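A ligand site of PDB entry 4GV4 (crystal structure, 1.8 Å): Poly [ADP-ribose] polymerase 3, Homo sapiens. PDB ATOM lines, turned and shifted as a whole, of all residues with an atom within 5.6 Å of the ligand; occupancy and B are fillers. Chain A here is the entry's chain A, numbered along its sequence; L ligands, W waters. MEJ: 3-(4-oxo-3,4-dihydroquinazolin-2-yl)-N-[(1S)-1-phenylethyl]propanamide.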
ATOM      1  N   ASP A 109     -10.043  10.769  28.606  1.00  0.00           N
ATOM      2  CA  ASP A 109      -9.314  11.965  29.069  1.00  0.00           C
ATOM      3  C   ASP A 109      -9.682  12.357  30.498  1.00  0.00           C
ATOM      4  O   ASP A 109      -8.814  12.792  31.267  1.00  0.00           O
ATOM      5  CB  ASP A 109      -9.602  13.124  28.141  1.00  0.00           C
ATOM      6  CG  ASP A 109      -8.904  12.987  26.800  1.00  0.00           C
ATOM      7  OD1 ASP A 109      -8.111  12.022  26.605  1.00  0.00           O
ATOM      8  OD2 ASP A 109      -9.134  13.871  25.917  1.00  0.00           O
ATOM      9  N   MET A 110     -10.968  12.233  30.834  1.00  0.00           N
ATOM     10  CA  MET A 110     -11.397  12.450  32.202  1.00  0.00           C
ATOM     11  C   MET A 110     -10.669  11.507  33.134  1.00  0.00           C
ATOM     12  O   MET A 110     -10.228  11.899  34.201  1.00  0.00           O
ATOM     13  CB  MET A 110     -12.923  12.258  32.344  1.00  0.00           C
ATOM     14  CG  MET A 110     -13.430  12.254  33.799  1.00  0.00           C
ATOM     15  SD  MET A 110     -13.216  10.718  34.704  1.00  0.00           S
ATOM     16  CE  MET A 110     -14.451   9.765  33.802  1.00  0.00           C
ATOM     17  N   LEU A 112      -7.759  10.012  32.694  1.00  0.00           N
ATOM     18  CA  LEU A 112      -6.351  10.409  32.749  1.00  0.00           C
ATOM     19  C   LEU A 112      -6.105  11.522  33.762  1.00  0.00           C
ATOM     20  O   LEU A 112      -5.110  11.491  34.512  1.00  0.00           O
ATOM     21  CB  LEU A 112      -5.863  10.840  31.352  1.00  0.00           C
ATOM     22  CG  LEU A 112      -5.757   9.646  30.363  1.00  0.00           C
ATOM     23  CD1 LEU A 112      -5.426  10.142  28.930  1.00  0.00           C
ATOM     24  CD2 LEU A 112      -4.685   8.677  30.843  1.00  0.00           C
ATOM     25  N   VAL A 113      -7.012  12.498  33.779  1.00  0.00           N
ATOM     26  CA  VAL A 113      -6.958  13.572  34.777  1.00  0.00           C
ATOM     27  C   VAL A 113      -7.188  12.982  36.170  1.00  0.00           C
ATOM     28  O   VAL A 113      -6.407  13.256  37.111  1.00  0.00           O
ATOM     29  CB  VAL A 113      -8.004  14.662  34.490  1.00  0.00           C
ATOM     30  CG1 VAL A 113      -8.043  15.711  35.626  1.00  0.00           C
ATOM     31  CG2 VAL A 113      -7.747  15.352  33.135  1.00  0.00           C
ATOM     32  N   ASP A 116      -4.186  11.308  37.653  1.00  0.00           N
ATOM     33  CA  ASP A 116      -3.203  12.254  38.140  1.00  0.00           C
ATOM     34  C   ASP A 116      -3.645  12.920  39.443  1.00  0.00           C
ATOM     35  O   ASP A 116      -2.823  13.298  40.252  1.00  0.00           O
ATOM     36  CB  ASP A 116      -2.825  13.315  37.084  1.00  0.00           C
ATOM     37  CG  ASP A 116      -1.867  12.765  36.018  1.00  0.00           C
ATOM     38  OD1 ASP A 116      -1.396  11.569  36.106  1.00  0.00           O
ATOM     39  OD2 ASP A 116      -1.498  13.581  35.159  1.00  0.00           O
ATOM     40  N   TRP A 208       4.601  25.397  23.778  1.00  0.00           N
ATOM     41  CA  TRP A 208       3.578  25.473  24.810  1.00  0.00           C
ATOM     42  C   TRP A 208       2.873  24.142  25.085  1.00  0.00           C
ATOM     43  O   TRP A 208       2.618  23.341  24.183  1.00  0.00           O
ATOM     44  CB  TRP A 208       2.529  26.497  24.466  1.00  0.00           C
ATOM     45  CG  TRP A 208       3.040  27.874  24.335  1.00  0.00           C
ATOM     46  CD1 TRP A 208       3.298  28.566  23.177  1.00  0.00           C
ATOM     47  CD2 TRP A 208       3.408  28.758  25.422  1.00  0.00           C
ATOM     48  NE1 TRP A 208       3.787  29.822  23.477  1.00  0.00           N
ATOM     49  CE2 TRP A 208       3.867  29.963  24.832  1.00  0.00           C
ATOM     50  CE3 TRP A 208       3.399  28.646  26.812  1.00  0.00           C
ATOM     51  CZ2 TRP A 208       4.311  31.044  25.601  1.00  0.00           C
ATOM     52  CZ3 TRP A 208       3.812  29.714  27.572  1.00  0.00           C
ATOM     53  CH2 TRP A 208       4.276  30.916  26.969  1.00  0.00           C
ATOM     54  N   HIS A 209       2.587  23.904  26.361  1.00  0.00           N
ATOM     55  CA  HIS A 209       1.737  22.803  26.781  1.00  0.00           C
ATOM     56  C   HIS A 209       0.833  23.287  27.884  1.00  0.00           C
ATOM     57  O   HIS A 209       1.289  23.563  28.992  1.00  0.00           O
ATOM     58  CB  HIS A 209       2.575  21.595  27.197  1.00  0.00           C
ATOM     59  CG  HIS A 209       1.761  20.391  27.496  1.00  0.00           C
ATOM     60  ND1 HIS A 209       1.358  19.482  26.522  1.00  0.00           N
ATOM     61  CD2 HIS A 209       1.311  19.892  28.674  1.00  0.00           C
ATOM     62  CE1 HIS A 209       0.655  18.525  27.082  1.00  0.00           C
ATOM     63  NE2 HIS A 209       0.610  18.741  28.389  1.00  0.00           N
ATOM     64  N   GLY A 210      -0.443  23.420  27.573  1.00  0.00           N
ATOM     65  CA  GLY A 210      -1.440  23.874  28.596  1.00  0.00           C
ATOM     66  C   GLY A 210      -2.153  22.682  29.201  1.00  0.00           C
ATOM     67  O   GLY A 210      -2.477  21.737  28.496  1.00  0.00           O
ATOM     68  N   THR A 211      -2.490  22.721  30.495  1.00  0.00           N
ATOM     69  CA  THR A 211      -3.172  21.630  31.169  1.00  0.00           C
ATOM     70  C   THR A 211      -4.154  22.053  32.271  1.00  0.00           C
ATOM     71  O   THR A 211      -4.163  23.152  32.574  1.00  0.00           O
ATOM     72  CB  THR A 211      -2.204  20.642  31.859  1.00  0.00           C
ATOM     73  OG1 THR A 211      -1.687  21.218  33.036  1.00  0.00           O
ATOM     74  CG2 THR A 211      -1.150  20.211  30.967  1.00  0.00           C
ATOM     75  N   ASN A 212      -4.949  21.107  32.752  1.00  0.00           N
ATOM     76  CA  ASN A 212      -5.726  21.237  33.952  1.00  0.00           C
ATOM     77  C   ASN A 212      -4.780  21.573  35.130  1.00  0.00           C
ATOM     78  O   ASN A 212      -3.794  20.992  35.279  1.00  0.00           O
ATOM     79  CB  ASN A 212      -6.390  19.892  34.350  1.00  0.00           C
ATOM     80  CG  ASN A 212      -7.753  19.654  33.737  1.00  0.00           C
ATOM     81  OD1 ASN A 212      -8.706  19.889  34.342  1.00  0.00           O
ATOM     82  ND2 ASN A 212      -7.798  19.119  32.583  1.00  0.00           N
ATOM     83  N   VAL A 215      -3.502  18.470  37.063  1.00  0.00           N
ATOM     84  CA  VAL A 215      -2.443  17.539  36.674  1.00  0.00           C
ATOM     85  C   VAL A 215      -1.019  18.164  36.780  1.00  0.00           C
ATOM     86  O   VAL A 215      -0.016  17.513  36.423  1.00  0.00           O
ATOM     87  CB  VAL A 215      -2.712  16.919  35.296  1.00  0.00           C
ATOM     88  CG1 VAL A 215      -4.125  16.333  35.188  1.00  0.00           C
ATOM     89  CG2 VAL A 215      -2.502  17.946  34.247  1.00  0.00           C
ATOM     90  N   ARG A 225       3.647  12.864  29.778  1.00  0.00           N
ATOM     91  CA  ARG A 225       3.562  11.425  29.583  1.00  0.00           C
ATOM     92  C   ARG A 225       2.626  11.046  28.430  1.00  0.00           C
ATOM     93  O   ARG A 225       1.713  11.810  28.064  1.00  0.00           O
ATOM     94  CB  ARG A 225       3.033  10.769  30.875  1.00  0.00           C
ATOM     95  CG  ARG A 225       4.118  10.767  31.992  1.00  0.00           C
ATOM     96  CD  ARG A 225       3.513  10.849  33.375  1.00  0.00           C
ATOM     97  NE  ARG A 225       2.852  12.148  33.522  1.00  0.00           N
ATOM     98  CZ  ARG A 225       1.700  12.359  34.137  1.00  0.00           C
ATOM     99  NH1 ARG A 225       1.033  11.375  34.768  1.00  0.00           N
ATOM    100  NH2 ARG A 225       1.206  13.576  34.105  1.00  0.00           N
ATOM    101  N   MET A 227       0.130   7.956  27.837  1.00  0.00           N
ATOM    102  CA  MET A 227      -0.545   6.866  28.574  1.00  0.00           C
ATOM    103  C   MET A 227      -1.272   5.915  27.577  1.00  0.00           C
ATOM    104  O   MET A 227      -1.492   6.287  26.405  1.00  0.00           O
ATOM    105  CB  MET A 227      -1.440   7.524  29.651  1.00  0.00           C
ATOM    106  CG  MET A 227      -0.777   8.819  30.369  1.00  0.00           C
ATOM    107  SD  MET A 227       0.444   8.383  31.661  1.00  0.00           S
ATOM    108  CE  MET A 227      -0.337   6.942  32.292  1.00  0.00           C
ATOM    109  N   SER A 230      -4.111   7.621  25.881  1.00  0.00           N
ATOM    110  CA  SER A 230      -3.878   8.974  25.270  1.00  0.00           C
ATOM    111  C   SER A 230      -4.397   8.998  23.846  1.00  0.00           C
ATOM    112  O   SER A 230      -4.240   8.007  23.144  1.00  0.00           O
ATOM    113  CB  SER A 230      -2.398   9.270  25.230  1.00  0.00           C
ATOM    114  OG  SER A 230      -1.893   9.449  26.508  1.00  0.00           O
ATOM    115  N   TYR A 239       1.168  16.365  22.977  1.00  0.00           N
ATOM    116  CA  TYR A 239       0.761  17.506  22.177  1.00  0.00           C
ATOM    117  C   TYR A 239       1.301  18.813  22.699  1.00  0.00           C
ATOM    118  O   TYR A 239       1.233  19.114  23.922  1.00  0.00           O
ATOM    119  CB  TYR A 239      -0.772  17.620  22.189  1.00  0.00           C
ATOM    120  CG  TYR A 239      -1.514  16.544  21.443  1.00  0.00           C
ATOM    121  CD1 TYR A 239      -2.101  16.799  20.207  1.00  0.00           C
ATOM    122  CD2 TYR A 239      -1.624  15.265  21.971  1.00  0.00           C
ATOM    123  CE1 TYR A 239      -2.776  15.802  19.525  1.00  0.00           C
ATOM    124  CE2 TYR A 239      -2.296  14.246  21.286  1.00  0.00           C
ATOM    125  CZ  TYR A 239      -2.869  14.519  20.067  1.00  0.00           C
ATOM    126  OH  TYR A 239      -3.527  13.516  19.376  1.00  0.00           O
ATOM    127  N   PHE A 240       1.841  19.585  21.771  1.00  0.00           N
ATOM    128  CA  PHE A 240       2.318  20.933  22.005  1.00  0.00           C
ATOM    129  C   PHE A 240       1.802  21.901  20.969  1.00  0.00           C
ATOM    130  O   PHE A 240       1.347  21.523  19.887  1.00  0.00           O
ATOM    131  CB  PHE A 240       3.854  21.004  21.971  1.00  0.00           C
ATOM    132  CG  PHE A 240       4.553  20.092  22.918  1.00  0.00           C
ATOM    133  CD1 PHE A 240       4.996  20.569  24.176  1.00  0.00           C
ATOM    134  CD2 PHE A 240       4.777  18.761  22.569  1.00  0.00           C
ATOM    135  CE1 PHE A 240       5.632  19.732  25.035  1.00  0.00           C
ATOM    136  CE2 PHE A 240       5.447  17.943  23.414  1.00  0.00           C
ATOM    137  CZ  PHE A 240       5.857  18.420  24.676  1.00  0.00           C
ATOM    138  N   ALA A 241       1.919  23.192  21.261  1.00  0.00           N
ATOM    139  CA  ALA A 241       1.577  24.237  20.273  1.00  0.00           C
ATOM    140  C   ALA A 241       2.657  25.309  20.242  1.00  0.00           C
ATOM    141  O   ALA A 241       3.266  25.597  21.272  1.00  0.00           O
ATOM    142  CB  ALA A 241       0.209  24.911  20.619  1.00  0.00           C
ATOM    143  N   LYS A 246      -3.494  28.550  21.251  1.00  0.00           N
ATOM    144  CA  LYS A 246      -3.902  27.146  21.103  1.00  0.00           C
ATOM    145  C   LYS A 246      -3.822  26.376  22.423  1.00  0.00           C
ATOM    146  O   LYS A 246      -4.819  25.759  22.884  1.00  0.00           O
ATOM    147  CB  LYS A 246      -3.064  26.451  20.005  1.00  0.00           C
ATOM    148  CG  LYS A 246      -3.377  24.986  19.833  1.00  0.00           C
ATOM    149  CD  LYS A 246      -4.785  24.772  19.231  1.00  0.00           C
ATOM    150  CE  LYS A 246      -5.120  23.323  19.048  1.00  0.00           C
ATOM    151  NZ  LYS A 246      -5.549  22.874  17.653  1.00  0.00           N
ATOM    152  N   SER A 247      -2.647  26.368  23.050  1.00  0.00           N
ATOM    153  CA  SER A 247      -2.466  25.701  24.320  1.00  0.00           C
ATOM    154  C   SER A 247      -3.337  26.249  25.423  1.00  0.00           C
ATOM    155  O   SER A 247      -3.731  25.549  26.345  1.00  0.00           O
ATOM    156  CB  SER A 247      -0.995  25.811  24.734  1.00  0.00           C
ATOM    157  OG  SER A 247      -0.271  24.869  23.957  1.00  0.00           O
ATOM    158  N   TYR A 250      -6.610  24.681  26.545  1.00  0.00           N
ATOM    159  CA  TYR A 250      -6.597  23.501  27.364  1.00  0.00           C
ATOM    160  C   TYR A 250      -6.336  23.783  28.812  1.00  0.00           C
ATOM    161  O   TYR A 250      -6.292  22.852  29.601  1.00  0.00           O
ATOM    162  CB  TYR A 250      -5.551  22.493  26.856  1.00  0.00           C
ATOM    163  CG  TYR A 250      -5.838  22.096  25.456  1.00  0.00           C
ATOM    164  CD1 TYR A 250      -6.682  21.019  25.184  1.00  0.00           C
ATOM    165  CD2 TYR A 250      -5.354  22.812  24.396  1.00  0.00           C
ATOM    166  CE1 TYR A 250      -6.972  20.639  23.863  1.00  0.00           C
ATOM    167  CE2 TYR A 250      -5.645  22.464  23.078  1.00  0.00           C
ATOM    168  CZ  TYR A 250      -6.447  21.356  22.840  1.00  0.00           C
ATOM    169  OH  TYR A 250      -6.742  21.061  21.527  1.00  0.00           O
ATOM    170  N   SER A 338      -1.202  24.986  14.540  1.00  0.00           N
ATOM    171  CA  SER A 338      -0.372  23.772  14.521  1.00  0.00           C
ATOM    172  C   SER A 338      -0.425  23.008  15.824  1.00  0.00           C
ATOM    173  O   SER A 338      -0.508  23.607  16.908  1.00  0.00           O
ATOM    174  CB  SER A 338       1.095  24.135  14.185  1.00  0.00           C
ATOM    175  OG  SER A 338       1.242  24.607  12.844  1.00  0.00           O
ATOM    176  N   GLU A 339      -0.369  21.669  15.715  1.00  0.00           N
ATOM    177  CA  GLU A 339      -0.172  20.790  16.844  1.00  0.00           C
ATOM    178  C   GLU A 339       1.107  20.012  16.575  1.00  0.00           C
ATOM    179  O   GLU A 339       1.234  19.360  15.501  1.00  0.00           O
ATOM    180  CB  GLU A 339      -1.338  19.818  17.040  1.00  0.00           C
ATOM    181  CG  GLU A 339      -2.737  20.563  17.075  1.00  0.00           C
ATOM    182  CD  GLU A 339      -3.902  19.741  17.489  1.00  0.00           C
ATOM    183  OE1 GLU A 339      -3.720  18.569  17.926  1.00  0.00           O
ATOM    184  OE2 GLU A 339      -5.048  20.279  17.420  1.00  0.00           O
HETATM  185  CAI MEJ L   1      -3.940  14.393  31.682  1.00  0.00           C
HETATM  186  CAE MEJ L   1      -3.078  13.503  32.272  1.00  0.00           C
HETATM  187  CAD MEJ L   1      -2.284  12.640  31.589  1.00  0.00           C
HETATM  188  CAF MEJ L   1      -2.350  12.639  30.193  1.00  0.00           C
HETATM  189  CAJ MEJ L   1      -3.203  13.533  29.544  1.00  0.00           C
HETATM  190  CAS MEJ L   1      -4.021  14.417  30.283  1.00  0.00           C
HETATM  191  CAX MEJ L   1      -4.962  15.400  29.657  1.00  0.00           C
HETATM  192  CAA MEJ L   1      -6.244  14.680  29.207  1.00  0.00           C
HETATM  193  NAP MEJ L   1      -4.320  16.010  28.465  1.00  0.00           N
HETATM  194  CAR MEJ L   1      -3.653  17.157  28.558  1.00  0.00           C
HETATM  195  OAB MEJ L   1      -3.412  17.742  29.606  1.00  0.00           O
HETATM  196  CAM MEJ L   1      -3.101  17.711  27.238  1.00  0.00           C
HETATM  197  CAN MEJ L   1      -3.756  19.065  26.990  1.00  0.00           C
HETATM  198  CAT MEJ L   1      -3.264  19.715  25.747  1.00  0.00           C
HETATM  199  NAO MEJ L   1      -3.665  19.291  24.540  1.00  0.00           N
HETATM  200  CAV MEJ L   1      -3.160  19.925  23.433  1.00  0.00           C
HETATM  201  CAK MEJ L   1      -3.592  19.486  22.172  1.00  0.00           C
HETATM  202  CAG MEJ L   1      -3.128  20.119  21.028  1.00  0.00           C
HETATM  203  CAH MEJ L   1      -2.254  21.199  21.167  1.00  0.00           C
HETATM  204  CAL MEJ L   1      -1.830  21.692  22.424  1.00  0.00           C
HETATM  205  CAW MEJ L   1      -2.284  21.023  23.539  1.00  0.00           C
HETATM  206  CAU MEJ L   1      -1.937  21.477  24.806  1.00  0.00           C
HETATM  207  OAC MEJ L   1      -1.207  22.457  25.002  1.00  0.00           O
HETATM  208  NAQ MEJ L   1      -2.437  20.778  25.895  1.00  0.00           N
HETATM  209  O   HOH W   1      -5.299  18.632  31.228  1.00  0.00           O
HETATM  210  O   HOH W   2      -4.281  14.661  25.665  1.00  0.00           O
HETATM  211  O   HOH W   3      -5.388  17.094  24.589  1.00  0.00           O
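N of Gly 210 sits at hydrogen-bond distance from OAC of the ligand (2.8 Å). A nitrogen (NAQ) of the ligand is in hydrogen-bond range of the backbone carbonyl oxygen (O) of Gly 210 (2.8 Å). An oxygen (OAC) of the ligand lies within hydrogen-bond range of the side-chain hydroxyl (OG) of Ser 247 (2.8 Å).
The side-chain hydroxyl of Ser 247 sits at hydrogen-bond distance from the backbone carbonyl oxygen of Trp 208 (3.3 Å). OD1 of Asp 116 is in salt-bridge range of NH1 of Arg 225, at 2.8 Å. O of Tyr 239 is in hydrogen-bond range of ND1 of His 209 (2.6 Å). NZ of Lys 246 lies within salt-bridge range of OE2 of Glu 339.
Asp 109 touches the ligand (O to CAA, 3.8 Å). O of Leu 112 touches CAE of the ligand, at 3.6 Å. OD2 of Asp 116 touches CAE of the ligand, at 3.3 Å. His 209 touches the ligand (CA to OAC, 3.5 Å). CG2 of Thr 211 touches OAB of the ligand, at 3.6 Å. Tyr 239 touches the ligand (CB to CAK, 3.4 Å). O of Phe 240 touches CAH of the ligand, 3.8 Å away. Tyr 250 touches the ligand (CZ to CAK, 3.5 Å). Glu 339 touches the ligand (OE1 to CAG, 3.5 Å). The nearest printed residue that does not touch the ligand is Trp 208 (4.01 Å).
Water W1 bridges OAB of the ligand and ND2 of Asn 212.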
